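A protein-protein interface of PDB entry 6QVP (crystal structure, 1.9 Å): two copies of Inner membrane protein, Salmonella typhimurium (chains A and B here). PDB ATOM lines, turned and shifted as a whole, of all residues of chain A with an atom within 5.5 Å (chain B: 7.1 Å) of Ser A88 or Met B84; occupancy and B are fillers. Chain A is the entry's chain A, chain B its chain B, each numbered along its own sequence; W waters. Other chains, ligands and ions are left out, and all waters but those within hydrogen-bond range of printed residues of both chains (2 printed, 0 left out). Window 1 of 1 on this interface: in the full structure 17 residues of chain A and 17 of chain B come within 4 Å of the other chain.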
ATOM      1  N   MET A  46      -3.716 -16.870   9.254  1.00  0.00           N
ATOM      2  CA  MET A  46      -2.798 -16.038   8.491  1.00  0.00           C
ATOM      3  C   MET A  46      -1.404 -16.647   8.631  1.00  0.00           C
ATOM      4  O   MET A  46      -0.919 -16.814   9.745  1.00  0.00           O
ATOM      5  CB  MET A  46      -2.839 -14.586   9.013  1.00  0.00           C
ATOM      6  CG  MET A  46      -4.234 -14.010   9.056  1.00  0.00           C
ATOM      7  SD  MET A  46      -5.086 -14.192   7.322  1.00  0.00           S
ATOM      8  CE  MET A  46      -3.427 -13.415   6.374  1.00  0.00           C
ATOM      9  N   ILE A  48       2.561 -16.193   7.890  1.00  0.00           N
ATOM     10  CA  ILE A  48       3.441 -15.049   7.621  1.00  0.00           C
ATOM     11  C   ILE A  48       4.901 -15.493   7.639  1.00  0.00           C
ATOM     12  O   ILE A  48       5.489 -15.686   8.694  1.00  0.00           O
ATOM     13  CB  ILE A  48       3.192 -13.905   8.622  1.00  0.00           C
ATOM     14  CG1 ILE A  48       1.694 -13.572   8.589  1.00  0.00           C
ATOM     15  CG2 ILE A  48       4.045 -12.711   8.232  1.00  0.00           C
ATOM     16  CD1 ILE A  48       1.159 -12.803   9.683  1.00  0.00           C
ATOM     17  N   PRO A  49       5.528 -15.636   6.477  1.00  0.00           N
ATOM     18  CA  PRO A  49       6.976 -15.938   6.448  1.00  0.00           C
ATOM     19  C   PRO A  49       7.809 -14.915   7.186  1.00  0.00           C
ATOM     20  O   PRO A  49       7.481 -13.722   7.235  1.00  0.00           O
ATOM     21  CB  PRO A  49       7.334 -15.898   4.949  1.00  0.00           C
ATOM     22  CG  PRO A  49       5.980 -16.120   4.199  1.00  0.00           C
ATOM     23  CD  PRO A  49       4.982 -15.412   5.117  1.00  0.00           C
ATOM     24  N   GLN A  50       8.947 -15.376   7.679  1.00  0.00           N
ATOM     25  CA  GLN A  50       9.794 -14.558   8.539  1.00  0.00           C
ATOM     26  C   GLN A  50      10.746 -13.738   7.675  1.00  0.00           C
ATOM     27  O   GLN A  50      11.657 -14.276   7.028  1.00  0.00           O
ATOM     28  CB  GLN A  50      10.542 -15.429   9.545  1.00  0.00           C
ATOM     29  CG  GLN A  50       9.574 -16.184  10.442  1.00  0.00           C
ATOM     30  CD  GLN A  50      10.248 -17.055  11.464  1.00  0.00           C
ATOM     31  OE1 GLN A  50      11.431 -17.448  11.338  1.00  0.00           O
ATOM     32  NE2 GLN A  50       9.521 -17.323  12.528  1.00  0.00           N
ATOM     33  N   LEU A  59       4.694  -8.736   9.545  1.00  0.00           N
ATOM     34  CA  LEU A  59       3.680  -9.153  10.503  1.00  0.00           C
ATOM     35  C   LEU A  59       2.461  -8.230  10.486  1.00  0.00           C
ATOM     36  O   LEU A  59       1.324  -8.691  10.467  1.00  0.00           O
ATOM     37  CB  LEU A  59       4.306  -9.229  11.881  1.00  0.00           C
ATOM     38  CG  LEU A  59       5.105 -10.510  12.147  1.00  0.00           C
ATOM     39  CD1 LEU A  59       5.928 -10.413  13.465  1.00  0.00           C
ATOM     40  CD2 LEU A  59       4.173 -11.716  12.206  1.00  0.00           C
ATOM     41  N   VAL A  86      -2.797 -16.941  13.773  1.00  0.00           N
ATOM     42  CA  VAL A  86      -1.613 -16.465  13.071  1.00  0.00           C
ATOM     43  C   VAL A  86      -0.493 -17.457  13.316  1.00  0.00           C
ATOM     44  O   VAL A  86      -0.324 -17.946  14.436  1.00  0.00           O
ATOM     45  CB  VAL A  86      -1.221 -15.052  13.557  1.00  0.00           C
ATOM     46  CG1 VAL A  86      -0.105 -14.454  12.734  1.00  0.00           C
ATOM     47  CG2 VAL A  86      -2.472 -14.141  13.584  1.00  0.00           C
ATOM     48  N   ASN A  87       0.268 -17.744  12.277  1.00  0.00           N
ATOM     49  CA  ASN A  87       1.507 -18.508  12.418  1.00  0.00           C
ATOM     50  C   ASN A  87       2.619 -17.878  11.583  1.00  0.00           C
ATOM     51  O   ASN A  87       2.443 -17.643  10.387  1.00  0.00           O
ATOM     52  CB  ASN A  87       1.302 -19.993  12.019  1.00  0.00           C
ATOM     53  CG  ASN A  87       2.485 -20.846  12.401  1.00  0.00           C
ATOM     54  OD1 ASN A  87       3.080 -20.681  13.497  1.00  0.00           O
ATOM     55  ND2 ASN A  87       2.832 -21.765  11.520  1.00  0.00           N
ATOM     56  N   SER A  88       3.756 -17.570  12.231  1.00  0.00           N
ATOM     57  CA  SER A  88       4.962 -17.034  11.559  1.00  0.00           C
ATOM     58  C   SER A  88       6.102 -17.961  11.982  1.00  0.00           C
ATOM     59  O   SER A  88       6.740 -17.751  13.033  1.00  0.00           O
ATOM     60  CB  SER A  88       5.316 -15.596  11.919  1.00  0.00           C
ATOM     61  OG  SER A  88       6.351 -15.138  11.062  1.00  0.00           O
ATOM     62  N   ALA A  89       6.329 -19.008  11.197  1.00  0.00           N
ATOM     63  CA  ALA A  89       7.269 -20.080  11.536  1.00  0.00           C
ATOM     64  C   ALA A  89       8.501 -19.970  10.654  1.00  0.00           C
ATOM     65  O   ALA A  89       8.450 -19.358   9.594  1.00  0.00           O
ATOM     66  CB  ALA A  89       6.595 -21.437  11.322  1.00  0.00           C
ATOM     67  N   ALA A  90       9.617 -20.553  11.093  1.00  0.00           N
ATOM     68  CA  ALA A  90      10.811 -20.601  10.239  1.00  0.00           C
ATOM     69  C   ALA A  90      10.567 -21.339   8.932  1.00  0.00           C
ATOM     70  O   ALA A  90      11.229 -21.053   7.930  1.00  0.00           O
ATOM     71  CB  ALA A  90      11.973 -21.268  10.985  1.00  0.00           C
ATOM     72  N   SER A  92       7.773 -21.445   7.153  1.00  0.00           N
ATOM     73  CA  SER A  92       6.793 -20.769   6.294  1.00  0.00           C
ATOM     74  C   SER A  92       7.464 -20.184   5.055  1.00  0.00           C
ATOM     75  O   SER A  92       8.323 -19.301   5.177  1.00  0.00           O
ATOM     76  CB  SER A  92       6.085 -19.649   7.073  1.00  0.00           C
ATOM     77  OG  SER A  92       5.507 -20.106   8.302  1.00  0.00           O
ATOM     78  N   LEU B  42      13.248 -22.000  19.620  1.00  0.00           N
ATOM     79  CA  LEU B  42      12.209 -21.461  20.476  1.00  0.00           C
ATOM     80  C   LEU B  42      10.866 -21.562  19.803  1.00  0.00           C
ATOM     81  O   LEU B  42      10.679 -21.085  18.676  1.00  0.00           O
ATOM     82  CB  LEU B  42      12.509 -19.996  20.834  1.00  0.00           C
ATOM     83  CG  LEU B  42      13.839 -19.815  21.555  1.00  0.00           C
ATOM     84  CD1 LEU B  42      14.106 -18.323  21.822  1.00  0.00           C
ATOM     85  CD2 LEU B  42      13.880 -20.571  22.871  1.00  0.00           C
ATOM     86  N   LEU B  43       9.929 -22.160  20.513  1.00  0.00           N
ATOM     87  CA  LEU B  43       8.543 -22.232  20.082  1.00  0.00           C
ATOM     88  C   LEU B  43       7.796 -21.195  20.913  1.00  0.00           C
ATOM     89  O   LEU B  43       7.794 -21.283  22.141  1.00  0.00           O
ATOM     90  CB  LEU B  43       7.994 -23.643  20.296  1.00  0.00           C
ATOM     91  CG  LEU B  43       6.603 -23.998  19.778  1.00  0.00           C
ATOM     92  CD1 LEU B  43       6.501 -23.756  18.295  1.00  0.00           C
ATOM     93  CD2 LEU B  43       6.266 -25.453  20.169  1.00  0.00           C
ATOM     94  N   ILE B  44       7.238 -20.168  20.266  1.00  0.00           N
ATOM     95  CA  ILE B  44       6.555 -19.106  20.980  1.00  0.00           C
ATOM     96  C   ILE B  44       5.071 -19.163  20.657  1.00  0.00           C
ATOM     97  O   ILE B  44       4.667 -19.187  19.484  1.00  0.00           O
ATOM     98  CB  ILE B  44       7.150 -17.735  20.651  1.00  0.00           C
ATOM     99  CG1 ILE B  44       8.604 -17.706  21.150  1.00  0.00           C
ATOM    100  CG2 ILE B  44       6.309 -16.627  21.264  1.00  0.00           C
ATOM    101  CD1 ILE B  44       9.295 -16.373  20.839  1.00  0.00           C
ATOM    102  N   GLU B  45       4.265 -19.131  21.704  1.00  0.00           N
ATOM    103  CA  GLU B  45       2.815 -19.051  21.570  1.00  0.00           C
ATOM    104  C   GLU B  45       2.345 -17.755  22.173  1.00  0.00           C
ATOM    105  O   GLU B  45       2.446 -17.554  23.384  1.00  0.00           O
ATOM    106  CB  GLU B  45       2.099 -20.188  22.291  1.00  0.00           C
ATOM    107  CG  GLU B  45       2.570 -21.547  22.071  1.00  0.00           C
ATOM    108  CD  GLU B  45       1.980 -22.470  23.138  1.00  0.00           C
ATOM    109  OE1 GLU B  45       0.745 -22.641  23.114  1.00  0.00           O
ATOM    110  OE2 GLU B  45       2.723 -22.900  24.053  1.00  0.00           O
ATOM    111  N   MET B  46       1.812 -16.892  21.355  1.00  0.00           N
ATOM    112  CA  MET B  46       1.107 -15.723  21.822  1.00  0.00           C
ATOM    113  C   MET B  46      -0.340 -16.169  22.046  1.00  0.00           C
ATOM    114  O   MET B  46      -0.988 -16.553  21.070  1.00  0.00           O
ATOM    115  CB  MET B  46       1.181 -14.600  20.773  1.00  0.00           C
ATOM    116  CG  MET B  46       2.624 -14.221  20.319  1.00  0.00           C
ATOM    117  SD  MET B  46       3.747 -13.791  21.882  1.00  0.00           S
ATOM    118  CE  MET B  46       2.532 -12.469  22.639  1.00  0.00           C
ATOM    119  N   GLY B  62      -1.711  -8.714  20.378  1.00  0.00           N
ATOM    120  CA  GLY B  62      -0.926  -9.936  20.342  1.00  0.00           C
ATOM    121  C   GLY B  62       0.168  -9.892  19.284  1.00  0.00           C
ATOM    122  O   GLY B  62       1.301 -10.295  19.537  1.00  0.00           O
ATOM    123  N   TYR B  63      -0.154  -9.360  18.097  1.00  0.00           N
ATOM    124  CA  TYR B  63       0.850  -9.133  17.060  1.00  0.00           C
ATOM    125  C   TYR B  63       1.977  -8.229  17.568  1.00  0.00           C
ATOM    126  O   TYR B  63       3.167  -8.496  17.346  1.00  0.00           O
ATOM    127  CB  TYR B  63       0.195  -8.479  15.837  1.00  0.00           C
ATOM    128  CG  TYR B  63      -0.337  -9.375  14.763  1.00  0.00           C
ATOM    129  CD1 TYR B  63       0.466  -9.778  13.683  1.00  0.00           C
ATOM    130  CD2 TYR B  63      -1.665  -9.719  14.746  1.00  0.00           C
ATOM    131  CE1 TYR B  63      -0.041 -10.530  12.653  1.00  0.00           C
ATOM    132  CE2 TYR B  63      -2.193 -10.534  13.717  1.00  0.00           C
ATOM    133  CZ  TYR B  63      -1.377 -10.934  12.700  1.00  0.00           C
ATOM    134  OH  TYR B  63      -1.947 -11.651  11.699  1.00  0.00           O
ATOM    135  N   ARG B  65       2.891  -7.446  20.621  1.00  0.00           N
ATOM    136  CA  ARG B  65       3.704  -7.994  21.704  1.00  0.00           C
ATOM    137  C   ARG B  65       4.605  -9.077  21.155  1.00  0.00           C
ATOM    138  O   ARG B  65       5.762  -9.179  21.550  1.00  0.00           O
ATOM    139  CB  ARG B  65       2.808  -8.494  22.841  1.00  0.00           C
ATOM    140  CG  ARG B  65       2.160  -7.334  23.619  1.00  0.00           C
ATOM    141  CD  ARG B  65       0.950  -7.773  24.502  1.00  0.00           C
ATOM    142  NE  ARG B  65       0.697  -6.781  25.548  1.00  0.00           N
ATOM    143  CZ  ARG B  65      -0.419  -6.677  26.264  1.00  0.00           C
ATOM    144  NH1 ARG B  65      -1.443  -7.486  26.060  1.00  0.00           N
ATOM    145  NH2 ARG B  65      -0.517  -5.741  27.190  1.00  0.00           N
ATOM    146  N   GLY B  66       4.127  -9.834  20.172  1.00  0.00           N
ATOM    147  CA  GLY B  66       5.004 -10.775  19.518  1.00  0.00           C
ATOM    148  C   GLY B  66       6.183 -10.077  18.871  1.00  0.00           C
ATOM    149  O   GLY B  66       7.314 -10.579  18.922  1.00  0.00           O
ATOM    150  N   ILE B  67       5.942  -8.913  18.244  1.00  0.00           N
ATOM    151  CA  ILE B  67       7.032  -8.158  17.611  1.00  0.00           C
ATOM    152  C   ILE B  67       8.047  -7.718  18.652  1.00  0.00           C
ATOM    153  O   ILE B  67       9.258  -7.907  18.480  1.00  0.00           O
ATOM    154  CB  ILE B  67       6.486  -6.961  16.814  1.00  0.00           C
ATOM    155  CG1 ILE B  67       5.877  -7.456  15.517  1.00  0.00           C
ATOM    156  CG2 ILE B  67       7.597  -5.991  16.423  1.00  0.00           C
ATOM    157  CD1 ILE B  67       4.953  -6.390  14.862  1.00  0.00           C
ATOM    158  N   LEU B  69       8.686  -9.065  21.485  1.00  0.00           N
ATOM    159  CA  LEU B  69       9.344 -10.202  22.110  1.00  0.00           C
ATOM    160  C   LEU B  69      10.398 -10.777  21.180  1.00  0.00           C
ATOM    161  O   LEU B  69      11.496 -11.131  21.621  1.00  0.00           O
ATOM    162  CB  LEU B  69       8.297 -11.259  22.484  1.00  0.00           C
ATOM    163  CG  LEU B  69       8.881 -12.548  23.047  1.00  0.00           C
ATOM    164  CD1 LEU B  69       9.840 -12.310  24.228  1.00  0.00           C
ATOM    165  CD2 LEU B  69       7.764 -13.472  23.497  1.00  0.00           C
ATOM    166  N   MET B  70      10.078 -10.887  19.891  1.00  0.00           N
ATOM    167  CA  MET B  70      11.049 -11.281  18.898  1.00  0.00           C
ATOM    168  C   MET B  70      12.255 -10.354  18.910  1.00  0.00           C
ATOM    169  O   MET B  70      13.410 -10.772  18.872  1.00  0.00           O
ATOM    170  CB  MET B  70      10.437 -11.275  17.503  1.00  0.00           C
ATOM    171  CG  MET B  70       9.490 -12.405  17.245  1.00  0.00           C
ATOM    172  SD  MET B  70       8.957 -12.484  15.374  1.00  0.00           S
ATOM    173  CE  MET B  70       8.595 -14.384  15.300  1.00  0.00           C
ATOM    174  N   ILE B  82      13.054 -19.169  15.633  1.00  0.00           N
ATOM    175  CA  ILE B  82      11.773 -18.985  16.310  1.00  0.00           C
ATOM    176  C   ILE B  82      10.666 -19.501  15.409  1.00  0.00           C
ATOM    177  O   ILE B  82      10.664 -19.237  14.200  1.00  0.00           O
ATOM    178  CB  ILE B  82      11.519 -17.494  16.644  1.00  0.00           C
ATOM    179  CG1 ILE B  82      12.599 -16.982  17.599  1.00  0.00           C
ATOM    180  CG2 ILE B  82      10.133 -17.306  17.282  1.00  0.00           C
ATOM    181  CD1 ILE B  82      12.596 -15.489  17.815  1.00  0.00           C
ATOM    182  N   ASP B  83       9.686 -20.186  16.020  1.00  0.00           N
ATOM    183  CA  ASP B  83       8.388 -20.432  15.417  1.00  0.00           C
ATOM    184  C   ASP B  83       7.383 -19.742  16.323  1.00  0.00           C
ATOM    185  O   ASP B  83       7.367 -19.998  17.533  1.00  0.00           O
ATOM    186  CB  ASP B  83       8.112 -21.942  15.310  1.00  0.00           C
ATOM    187  CG  ASP B  83       9.142 -22.665  14.441  1.00  0.00           C
ATOM    188  OD1 ASP B  83       9.270 -22.308  13.253  1.00  0.00           O
ATOM    189  OD2 ASP B  83       9.800 -23.611  14.936  1.00  0.00           O
ATOM    190  N   MET B  84       6.595 -18.834  15.776  1.00  0.00           N
ATOM    191  CA  MET B  84       5.672 -18.076  16.620  1.00  0.00           C
ATOM    192  C   MET B  84       4.257 -18.035  16.109  1.00  0.00           C
ATOM    193  O   MET B  84       3.985 -17.755  14.904  1.00  0.00           O
ATOM    194  CB  MET B  84       6.166 -16.657  16.807  1.00  0.00           C
ATOM    195  CG  MET B  84       5.233 -15.875  17.738  1.00  0.00           C
ATOM    196  SD  MET B  84       5.890 -14.052  18.026  1.00  0.00           S
ATOM    197  CE  MET B  84       5.342 -13.101  16.476  1.00  0.00           C
ATOM    198  N   SER B  85       3.330 -18.304  17.022  1.00  0.00           N
ATOM    199  CA  SER B  85       1.917 -18.330  16.671  1.00  0.00           C
ATOM    200  C   SER B  85       1.124 -17.339  17.508  1.00  0.00           C
ATOM    201  O   SER B  85       1.507 -16.993  18.615  1.00  0.00           O
ATOM    202  CB  SER B  85       1.295 -19.743  16.873  1.00  0.00           C
ATOM    203  OG  SER B  85       1.363 -20.181  18.241  1.00  0.00           O
ATOM    204  N   VAL B  86      -0.069 -17.001  17.020  1.00  0.00           N
ATOM    205  CA  VAL B  86      -1.047 -16.239  17.783  1.00  0.00           C
ATOM    206  C   VAL B  86      -2.402 -16.938  17.714  1.00  0.00           C
ATOM    207  O   VAL B  86      -2.938 -17.169  16.616  1.00  0.00           O
ATOM    208  CB  VAL B  86      -1.177 -14.788  17.269  1.00  0.00           C
ATOM    209  CG1 VAL B  86      -1.886 -13.949  18.275  1.00  0.00           C
ATOM    210  CG2 VAL B  86       0.226 -14.172  16.987  1.00  0.00           C
ATOM    211  N   ASN B  87      -2.989 -17.199  18.879  1.00  0.00           N
ATOM    212  CA  ASN B  87      -4.260 -17.897  18.969  1.00  0.00           C
ATOM    213  C   ASN B  87      -5.086 -17.365  20.120  1.00  0.00           C
ATOM    214  O   ASN B  87      -4.549 -16.881  21.118  1.00  0.00           O
ATOM    215  CB  ASN B  87      -4.033 -19.407  19.130  1.00  0.00           C
ATOM    216  CG  ASN B  87      -3.467 -20.035  17.901  1.00  0.00           C
ATOM    217  OD1 ASN B  87      -4.214 -20.368  16.993  1.00  0.00           O
ATOM    218  ND2 ASN B  87      -2.154 -20.239  17.852  1.00  0.00           N
HETATM  219  O   HOH W   1       9.332 -23.920  11.475  1.00  0.00           O
HETATM  220  O   HOH W   2      13.203 -17.746  13.317  1.00  0.00           O
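N of Ser A88 sits at hydrogen-bond distance from O of Met B84 (2.7 Å).
The side-chain amide oxygen (OD1) of Asn A87 lies close to the backbone carbonyl oxygen (O) of Met B84.
N of Val B86 sits at hydrogen-bond distance from O of Val A86 (2.8 Å).
N of Ala A90 lies within hydrogen-bond range of OD1 of Asp B83, 2.8 Å away.
NE2 of Gln A50 sits at hydrogen-bond distance from O of Ile B82 (2.8 Å).
Among the printed residues, merely in contact across the chains: Ile A48 with Tyr B63 (3.9 Å), Leu A59 with Tyr B63 (3.2 Å), Leu A59 with Ile B67 (3.6 Å), Val A86 with Tyr B63 (3.2 Å), Val A86 with Ser B85 (3.2 Å), Asn A87 with Ser B85 (3.9 Å), Ser A88 with Asp B83 (3.9 Å), Ala A89 with Asp B83 (3.4 Å) and Ala A90 with Ile B82 (3.5 Å).
Val A86 touches its own counterpart, Val B86.
Of chain B, only Asp B83 and Met B84 come within 4 Å of Ser A88.
Met B84 touches two residues of chain A.
Printed residues of chain B within 4 Å of Asn A87: Met B84 and Ser B85.
Printed residues of chain B within 4 Å of Ile A48: Tyr B63 (3.9 Å).
Printed residues of chain A within 4 Å of Ile B82: Gln A50 (2.8 Å) and Ala A90 (3.5 Å).
The nearest printed residue of chain B that does not touch Ala A89 is Ile B82 (4.2 Å).
The backbone NH of Ser B85 sits at hydrogen-bond distance from the backbone carbonyl oxygen of Ile B44, 2.9 Å away.
The backbone carbonyl oxygen of Ser A88 sits at hydrogen-bond distance from the side-chain amide nitrogen of Gln A50 (2.9 Å).
O of Met A46 lies within hydrogen-bond range of N of Asn A87 (2.9 Å).
The backbone NH (N) of Met B46 lies within hydrogen-bond range of the backbone carbonyl oxygen (O) of Ser B85, 2.8 Å away.
N of Asp B83 sits at hydrogen-bond distance from O of Leu B42, at 3.0 Å.
The backbone NH (N) of Ala A89 lies within hydrogen-bond range of the side-chain hydroxyl (OG) of Ser A92, at 3.2 Å.
Water W1 bridges OD1 of Asp B83 (2.4 Å) and N of Ala A90 (3.4 Å).
Water W2 lies within hydrogen-bond range of OE1 of Gln A50 and N of Ile B82.
Of the 18 printed residues of chain B, 7 touch a printed residue of chain A.
Along chain B the printed residues that touch a printed residue of chain A span positions 63 to 86.
Of the 11 printed residues of chain A, 8 touch a printed residue of chain B.
Printed residues of chain A that touch a printed residue of chain B: Ile A48, Gln A50, Leu A59, Val A86, Asn A87, Ser A88, Ala A89 and Ala A90.
Hydrophobic or aromatic side chains of chain A that line the printed part of chain B: Ile A48, Leu A59, Val A86, Ala A89 and Ala A90.
Along chain A the printed residues that touch a printed residue of chain B span positions 48 to 90.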
